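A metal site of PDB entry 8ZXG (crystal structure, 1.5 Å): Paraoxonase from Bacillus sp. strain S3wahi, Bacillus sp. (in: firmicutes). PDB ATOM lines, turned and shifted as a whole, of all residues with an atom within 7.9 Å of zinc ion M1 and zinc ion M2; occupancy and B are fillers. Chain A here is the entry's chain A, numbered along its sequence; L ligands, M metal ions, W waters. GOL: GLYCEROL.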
ATOM      1  N   VAL A  11     -19.726   2.890  12.157  1.00  0.00           N
ATOM      2  CA  VAL A  11     -19.179   3.960  11.322  1.00  0.00           C
ATOM      3  C   VAL A  11     -20.324   4.852  10.892  1.00  0.00           C
ATOM      4  O   VAL A  11     -21.467   4.385  10.812  1.00  0.00           O
ATOM      5  CB  VAL A  11     -18.385   3.410  10.113  1.00  0.00           C
ATOM      6  CG1 VAL A  11     -17.179   2.617  10.605  1.00  0.00           C
ATOM      7  CG2 VAL A  11     -19.254   2.535   9.225  1.00  0.00           C
ATOM      8  N   PHE A  13     -21.402   5.986   8.207  1.00  0.00           N
ATOM      9  CA  PHE A  13     -21.664   5.779   6.800  1.00  0.00           C
ATOM     10  C   PHE A  13     -22.872   4.862   6.641  1.00  0.00           C
ATOM     11  O   PHE A  13     -23.277   4.208   7.601  1.00  0.00           O
ATOM     12  CB  PHE A  13     -20.450   5.129   6.129  1.00  0.00           C
ATOM     13  CG  PHE A  13     -19.141   5.906   6.261  1.00  0.00           C
ATOM     14  CD1 PHE A  13     -19.081   7.275   6.144  1.00  0.00           C
ATOM     15  CD2 PHE A  13     -17.962   5.230   6.404  1.00  0.00           C
ATOM     16  CE1 PHE A  13     -17.864   7.953   6.257  1.00  0.00           C
ATOM     17  CE2 PHE A  13     -16.742   5.900   6.497  1.00  0.00           C
ATOM     18  CZ  PHE A  13     -16.695   7.256   6.427  1.00  0.00           C
ATOM     19  N   VAL A  15     -23.247   2.022   5.405  1.00  0.00           N
ATOM     20  CA  VAL A  15     -22.966   0.618   5.683  1.00  0.00           C
ATOM     21  C   VAL A  15     -23.078   0.301   7.191  1.00  0.00           C
ATOM     22  O   VAL A  15     -23.126  -0.875   7.592  1.00  0.00           O
ATOM     23  CB  VAL A  15     -21.588   0.272   5.114  1.00  0.00           C
ATOM     24  CG1 VAL A  15     -20.433   0.825   5.956  1.00  0.00           C
ATOM     25  CG2 VAL A  15     -21.434  -1.226   4.944  1.00  0.00           C
ATOM     26  N   THR A  17     -21.643  -0.386   9.849  1.00  0.00           N
ATOM     27  CA  THR A  17     -20.614  -1.076  10.635  1.00  0.00           C
ATOM     28  C   THR A  17     -19.508  -1.476   9.688  1.00  0.00           C
ATOM     29  O   THR A  17     -19.746  -1.760   8.528  1.00  0.00           O
ATOM     30  CB  THR A  17     -21.096  -2.309  11.403  1.00  0.00           C
ATOM     31  OG1 THR A  17     -21.501  -3.298  10.504  1.00  0.00           O
ATOM     32  CG2 THR A  17     -22.248  -1.899  12.288  1.00  0.00           C
ATOM     33  N   VAL A  18     -18.298  -1.547  10.232  1.00  0.00           N
ATOM     34  CA  VAL A  18     -17.152  -2.141   9.579  1.00  0.00           C
ATOM     35  C   VAL A  18     -16.726  -3.335  10.433  1.00  0.00           C
ATOM     36  O   VAL A  18     -16.809  -3.285  11.674  1.00  0.00           O
ATOM     37  CB  VAL A  18     -15.984  -1.153   9.372  1.00  0.00           C
ATOM     38  CG1 VAL A  18     -15.378  -0.652  10.676  1.00  0.00           C
ATOM     39  CG2 VAL A  18     -14.908  -1.736   8.487  1.00  0.00           C
ATOM     40  N   ASN A  19     -16.286  -4.403   9.773  1.00  0.00           N
ATOM     41  CA  ASN A  19     -15.756  -5.554  10.470  1.00  0.00           C
ATOM     42  C   ASN A  19     -14.254  -5.377  10.617  1.00  0.00           C
ATOM     43  O   ASN A  19     -13.566  -5.165   9.601  1.00  0.00           O
ATOM     44  CB  ASN A  19     -16.009  -6.837   9.722  1.00  0.00           C
ATOM     45  CG  ASN A  19     -17.473  -7.148   9.554  1.00  0.00           C
ATOM     46  OD1 ASN A  19     -18.291  -6.848  10.451  1.00  0.00           O
ATOM     47  ND2 ASN A  19     -17.792  -7.811   8.432  1.00  0.00           N
ATOM     48  N   ASP A  32      -7.742  -3.735  10.255  1.00  0.00           N
ATOM     49  CA  ASP A  32      -8.679  -2.620  10.087  1.00  0.00           C
ATOM     50  C   ASP A  32      -9.118  -2.053  11.434  1.00  0.00           C
ATOM     51  O   ASP A  32      -8.960  -2.708  12.467  1.00  0.00           O
ATOM     52  CB  ASP A  32      -9.774  -2.984   9.098  1.00  0.00           C
ATOM     53  CG  ASP A  32      -9.290  -3.195   7.684  1.00  0.00           C
ATOM     54  OD1 ASP A  32      -8.125  -2.744   7.387  1.00  0.00           O
ATOM     55  OD2 ASP A  32     -10.056  -3.735   6.864  1.00  0.00           O
ATOM     56  N   THR A  64      -6.354  -3.193   5.235  1.00  0.00           N
ATOM     57  CA  THR A  64      -6.715  -3.703   3.938  1.00  0.00           C
ATOM     58  C   THR A  64      -6.683  -2.612   2.878  1.00  0.00           C
ATOM     59  O   THR A  64      -6.390  -2.896   1.712  1.00  0.00           O
ATOM     60  CB  THR A  64      -8.082  -4.413   3.921  1.00  0.00           C
ATOM     61  OG1 THR A  64      -9.111  -3.474   4.316  1.00  0.00           O
ATOM     62  CG2 THR A  64      -8.095  -5.622   4.823  1.00  0.00           C
ATOM     63  N   HIS A  65      -7.015  -1.368   3.266  1.00  0.00           N
ATOM     64  CA  HIS A  65      -6.989  -0.230   2.352  1.00  0.00           C
ATOM     65  C   HIS A  65      -7.153   1.079   3.125  1.00  0.00           C
ATOM     66  O   HIS A  65      -7.359   1.067   4.322  1.00  0.00           O
ATOM     67  CB  HIS A  65      -8.042  -0.415   1.240  1.00  0.00           C
ATOM     68  CG  HIS A  65      -9.476  -0.451   1.646  1.00  0.00           C
ATOM     69  ND1 HIS A  65     -10.003  -1.366   2.527  1.00  0.00           N
ATOM     70  CD2 HIS A  65     -10.525   0.318   1.220  1.00  0.00           C
ATOM     71  CE1 HIS A  65     -11.318  -1.200   2.584  1.00  0.00           C
ATOM     72  NE2 HIS A  65     -11.649  -0.195   1.791  1.00  0.00           N
ATOM     73  N   HIS A  66      -7.066   2.213   2.390  1.00  0.00           N
ATOM     74  CA  HIS A  66      -6.957   3.525   3.013  1.00  0.00           C
ATOM     75  C   HIS A  66      -8.305   4.172   3.363  1.00  0.00           C
ATOM     76  O   HIS A  66      -8.326   5.239   3.958  1.00  0.00           O
ATOM     77  CB  HIS A  66      -6.243   4.466   2.055  1.00  0.00           C
ATOM     78  CG  HIS A  66      -7.050   4.859   0.847  1.00  0.00           C
ATOM     79  ND1 HIS A  66      -6.969   4.197  -0.345  1.00  0.00           N
ATOM     80  CD2 HIS A  66      -7.885   5.905   0.647  1.00  0.00           C
ATOM     81  CE1 HIS A  66      -7.752   4.769  -1.235  1.00  0.00           C
ATOM     82  NE2 HIS A  66      -8.324   5.818  -0.640  1.00  0.00           N
ATOM     83  N   HIS A  67      -9.419   3.516   2.998  1.00  0.00           N
ATOM     84  CA  HIS A  67     -10.706   4.132   3.289  1.00  0.00           C
ATOM     85  C   HIS A  67     -10.840   4.343   4.807  1.00  0.00           C
ATOM     86  O   HIS A  67     -10.364   3.564   5.599  1.00  0.00           O
ATOM     87  CB  HIS A  67     -11.851   3.297   2.728  1.00  0.00           C
ATOM     88  CG  HIS A  67     -11.919   3.247   1.244  1.00  0.00           C
ATOM     89  ND1 HIS A  67     -12.729   2.409   0.528  1.00  0.00           N
ATOM     90  CD2 HIS A  67     -11.268   4.021   0.321  1.00  0.00           C
ATOM     91  CE1 HIS A  67     -12.582   2.669  -0.759  1.00  0.00           C
ATOM     92  NE2 HIS A  67     -11.685   3.653  -0.918  1.00  0.00           N
ATOM     93  N   ALA A  68     -11.469   5.451   5.187  1.00  0.00           N
ATOM     94  CA  ALA A  68     -11.486   5.915   6.565  1.00  0.00           C
ATOM     95  C   ALA A  68     -12.079   4.925   7.560  1.00  0.00           C
ATOM     96  O   ALA A  68     -11.659   4.904   8.732  1.00  0.00           O
ATOM     97  CB  ALA A  68     -12.248   7.227   6.659  1.00  0.00           C
ATOM     98  N   ASP A  69     -13.036   4.101   7.087  1.00  0.00           N
ATOM     99  CA  ASP A  69     -13.605   3.090   7.962  1.00  0.00           C
ATOM    100  C   ASP A  69     -12.603   1.977   8.341  1.00  0.00           C
ATOM    101  O   ASP A  69     -12.835   1.251   9.317  1.00  0.00           O
ATOM    102  CB  ASP A  69     -14.908   2.546   7.405  1.00  0.00           C
ATOM    103  CG  ASP A  69     -14.945   2.189   5.917  1.00  0.00           C
ATOM    104  OD1 ASP A  69     -14.345   2.802   4.939  1.00  0.00           O
ATOM    105  OD2 ASP A  69     -15.594   1.143   5.595  1.00  0.00           O
ATOM    106  N   HIS A  70     -11.501   1.873   7.589  1.00  0.00           N
ATOM    107  CA  HIS A  70     -10.506   0.836   7.817  1.00  0.00           C
ATOM    108  C   HIS A  70      -9.230   1.339   8.510  1.00  0.00           C
ATOM    109  O   HIS A  70      -8.547   0.544   9.113  1.00  0.00           O
ATOM    110  CB  HIS A  70     -10.237   0.092   6.521  1.00  0.00           C
ATOM    111  CG  HIS A  70     -11.478  -0.507   5.933  1.00  0.00           C
ATOM    112  ND1 HIS A  70     -11.840  -1.816   6.095  1.00  0.00           N
ATOM    113  CD2 HIS A  70     -12.480   0.086   5.291  1.00  0.00           C
ATOM    114  CE1 HIS A  70     -13.029  -2.021   5.558  1.00  0.00           C
ATOM    115  NE2 HIS A  70     -13.435  -0.863   5.047  1.00  0.00           N
ATOM    116  N   HIS A 163     -11.532  -1.835  -5.800  1.00  0.00           N
ATOM    117  CA  HIS A 163     -12.279  -1.097  -4.815  1.00  0.00           C
ATOM    118  C   HIS A 163     -11.500   0.148  -4.396  1.00  0.00           C
ATOM    119  O   HIS A 163     -12.080   1.218  -4.204  1.00  0.00           O
ATOM    120  CB  HIS A 163     -12.576  -1.970  -3.597  1.00  0.00           C
ATOM    121  CG  HIS A 163     -13.266  -1.238  -2.505  1.00  0.00           C
ATOM    122  ND1 HIS A 163     -14.599  -0.909  -2.545  1.00  0.00           N
ATOM    123  CD2 HIS A 163     -12.810  -0.778  -1.333  1.00  0.00           C
ATOM    124  CE1 HIS A 163     -14.937  -0.272  -1.417  1.00  0.00           C
ATOM    125  NE2 HIS A 163     -13.870  -0.206  -0.661  1.00  0.00           N
ATOM    126  N   ALA A 164     -10.205  -0.008  -4.220  1.00  0.00           N
ATOM    127  CA  ALA A 164      -9.271   1.081  -3.940  1.00  0.00           C
ATOM    128  C   ALA A 164      -7.916   0.675  -4.488  1.00  0.00           C
ATOM    129  O   ALA A 164      -7.615  -0.505  -4.570  1.00  0.00           O
ATOM    130  CB  ALA A 164      -9.166   1.329  -2.454  1.00  0.00           C
ATOM    131  N   HIS A 167      -5.774  -1.503  -2.104  1.00  0.00           N
ATOM    132  CA  HIS A 167      -6.488  -2.650  -1.532  1.00  0.00           C
ATOM    133  C   HIS A 167      -5.663  -3.935  -1.567  1.00  0.00           C
ATOM    134  O   HIS A 167      -5.208  -4.349  -2.621  1.00  0.00           O
ATOM    135  CB  HIS A 167      -7.856  -2.820  -2.212  1.00  0.00           C
ATOM    136  CG  HIS A 167      -8.804  -3.552  -1.368  1.00  0.00           C
ATOM    137  ND1 HIS A 167      -8.771  -4.926  -1.208  1.00  0.00           N
ATOM    138  CD2 HIS A 167      -9.712  -3.080  -0.471  1.00  0.00           C
ATOM    139  CE1 HIS A 167      -9.677  -5.254  -0.305  1.00  0.00           C
ATOM    140  NE2 HIS A 167     -10.263  -4.149   0.157  1.00  0.00           N
ATOM    141  N   GLY A 181     -11.105  -7.694   3.171  1.00  0.00           N
ATOM    142  CA  GLY A 181     -11.374  -6.274   3.030  1.00  0.00           C
ATOM    143  C   GLY A 181     -12.687  -6.042   2.308  1.00  0.00           C
ATOM    144  O   GLY A 181     -13.642  -6.809   2.489  1.00  0.00           O
ATOM    145  N   ASP A 182     -12.699  -5.006   1.450  1.00  0.00           N
ATOM    146  CA  ASP A 182     -13.872  -4.636   0.699  1.00  0.00           C
ATOM    147  C   ASP A 182     -13.866  -5.133  -0.746  1.00  0.00           C
ATOM    148  O   ASP A 182     -14.664  -4.689  -1.557  1.00  0.00           O
ATOM    149  CB  ASP A 182     -14.099  -3.141   0.780  1.00  0.00           C
ATOM    150  CG  ASP A 182     -14.492  -2.572   2.148  1.00  0.00           C
ATOM    151  OD1 ASP A 182     -14.603  -3.431   3.102  1.00  0.00           O
ATOM    152  OD2 ASP A 182     -14.621  -1.294   2.257  1.00  0.00           O
ATOM    153  N   ALA A 183     -12.989  -6.082  -1.076  1.00  0.00           N
ATOM    154  CA  ALA A 183     -12.896  -6.567  -2.438  1.00  0.00           C
ATOM    155  C   ALA A 183     -14.170  -7.288  -2.867  1.00  0.00           C
ATOM    156  O   ALA A 183     -14.576  -7.120  -4.014  1.00  0.00           O
ATOM    157  CB  ALA A 183     -11.711  -7.453  -2.627  1.00  0.00           C
ATOM    158  N   ILE A 185     -17.968  -8.017  -1.068  1.00  0.00           N
ATOM    159  CA  ILE A 185     -18.932  -7.870   0.010  1.00  0.00           C
ATOM    160  C   ILE A 185     -20.219  -8.582  -0.401  1.00  0.00           C
ATOM    161  O   ILE A 185     -20.682  -8.428  -1.532  1.00  0.00           O
ATOM    162  CB  ILE A 185     -19.145  -6.377   0.300  1.00  0.00           C
ATOM    163  CG1 ILE A 185     -17.838  -5.729   0.721  1.00  0.00           C
ATOM    164  CG2 ILE A 185     -20.229  -6.163   1.353  1.00  0.00           C
ATOM    165  CD1 ILE A 185     -17.921  -4.227   0.765  1.00  0.00           C
ATOM    166  N   SER A 190     -19.013  -3.492  -4.343  1.00  0.00           N
ATOM    167  CA  SER A 190     -17.921  -2.746  -3.740  1.00  0.00           C
ATOM    168  C   SER A 190     -17.117  -2.083  -4.851  1.00  0.00           C
ATOM    169  O   SER A 190     -15.883  -2.077  -4.812  1.00  0.00           O
ATOM    170  CB  SER A 190     -17.019  -3.641  -2.885  1.00  0.00           C
ATOM    171  OG  SER A 190     -16.903  -4.939  -3.401  1.00  0.00           O
ATOM    172  N   ASN A 191     -17.845  -1.508  -5.841  1.00  0.00           N
ATOM    173  CA  ASN A 191     -17.251  -1.091  -7.092  1.00  0.00           C
ATOM    174  C   ASN A 191     -16.221  -0.002  -6.820  1.00  0.00           C
ATOM    175  O   ASN A 191     -16.262   0.610  -5.787  1.00  0.00           O
ATOM    176  CB  ASN A 191     -18.320  -0.564  -8.023  1.00  0.00           C
ATOM    177  CG  ASN A 191     -19.015  -1.708  -8.744  1.00  0.00           C
ATOM    178  OD1 ASN A 191     -18.634  -2.880  -8.580  1.00  0.00           O
ATOM    179  ND2 ASN A 191     -19.995  -1.384  -9.555  1.00  0.00           N
ATOM    180  N   ILE A 193     -14.169   3.097  -5.966  1.00  0.00           N
ATOM    181  CA  ILE A 193     -14.346   4.417  -5.401  1.00  0.00           C
ATOM    182  C   ILE A 193     -13.323   5.362  -6.038  1.00  0.00           C
ATOM    183  O   ILE A 193     -12.128   5.085  -5.955  1.00  0.00           O
ATOM    184  CB  ILE A 193     -14.162   4.337  -3.868  1.00  0.00           C
ATOM    185  CG1 ILE A 193     -15.111   3.280  -3.211  1.00  0.00           C
ATOM    186  CG2 ILE A 193     -14.273   5.724  -3.231  1.00  0.00           C
ATOM    187  CD1 ILE A 193     -16.556   3.490  -3.554  1.00  0.00           C
ATOM    188  N   GLY A 229     -14.941  -6.968   4.928  1.00  0.00           N
ATOM    189  CA  GLY A 229     -14.873  -5.712   5.651  1.00  0.00           C
ATOM    190  C   GLY A 229     -16.234  -5.238   6.130  1.00  0.00           C
ATOM    191  O   GLY A 229     -16.299  -4.461   7.055  1.00  0.00           O
ATOM    192  N   HIS A 230     -17.313  -5.705   5.457  1.00  0.00           N
ATOM    193  CA  HIS A 230     -18.654  -5.344   5.830  1.00  0.00           C
ATOM    194  C   HIS A 230     -19.590  -6.513   5.647  1.00  0.00           C
ATOM    195  O   HIS A 230     -19.479  -7.241   4.685  1.00  0.00           O
ATOM    196  CB  HIS A 230     -19.163  -4.146   5.028  1.00  0.00           C
ATOM    197  CG  HIS A 230     -18.277  -2.949   5.088  1.00  0.00           C
ATOM    198  ND1 HIS A 230     -18.318  -2.067   6.150  1.00  0.00           N
ATOM    199  CD2 HIS A 230     -17.308  -2.536   4.277  1.00  0.00           C
ATOM    200  CE1 HIS A 230     -17.357  -1.136   5.951  1.00  0.00           C
ATOM    201  NE2 HIS A 230     -16.733  -1.432   4.822  1.00  0.00           N
HETATM  202  C1  GOL L   1     -18.518   1.095  -0.523  1.00  0.00           C
HETATM  203  O1  GOL L   1     -19.881   1.429  -0.786  1.00  0.00           O
HETATM  204  C2  GOL L   1     -18.321   0.610   0.893  1.00  0.00           C
HETATM  205  O2  GOL L   1     -19.238   1.235   1.788  1.00  0.00           O
HETATM  206  C3  GOL L   1     -16.918   0.791   1.428  1.00  0.00           C
HETATM  207  O3  GOL L   1     -16.865   0.507   2.823  1.00  0.00           O
HETATM  208 ZN    ZN M   1     -13.669   0.593   1.278  1.00  0.00          ZN
HETATM  209 ZN    ZN M   2     -15.207  -0.271   3.971  1.00  0.00          ZN
HETATM  210 MG    MG M   3     -10.792   4.651  -3.386  1.00  0.00          MG
HETATM  211 MG    MG M   4     -10.694   7.030  -1.764  1.00  0.00          MG
HETATM  212  O   HOH W   1     -14.243   1.378   3.246  1.00  0.00           O
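Zinc ion M1 is bound by NE2 of His 163 (2.1 Å), ND1 of His 67 (2.2 Å), water W1 (2.2 Å), NE2 of His 65 (2.2 Å) and OD2 of Asp 182 (2.3 Å).
Zinc ion M2 is bound by water W1 (2.0 Å), OD2 of Asp 182 (2.1 Å), NE2 of His 230 (2.1 Å), NE2 of His 70 (2.2 Å), O3 of the ligand (2.2 Å) and OD2 of Asp 69 (2.2 Å).
N of Asp 182 is in hydrogen-bond range of NE2 of His 167.
O of Asp 182 sits close to OG of Ser 190, at 2.9 Å.
O of Thr 17 is in hydrogen-bond range of ND1 of His 230, 2.8 Å away.
N of Ile 193 sits at hydrogen-bond distance from O of His 163.
ND1 of His 163 sits at hydrogen-bond distance from O of Ser 190, at 2.9 Å.
A ring nitrogen (ND1) of His 70 lies within hydrogen-bond range of the side-chain carboxylate (OD2) of Asp 32 (2.7 Å).
ND1 of His 65 lies within hydrogen-bond range of OG1 of Thr 64 (2.9 Å).
Four residues have an atom within 4 Å of zinc ion M2: Asp 69, His 70, Asp 182 and His 230.
Along chain A the residues within 4 Å of zinc ion M2 span positions 69 to 230.
The nearest printed residue that does not touch zinc ion M2 is His 65 (4.2 Å).
The nearest printed residue that does not touch zinc ion M1 is His 70 (4.05 Å).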
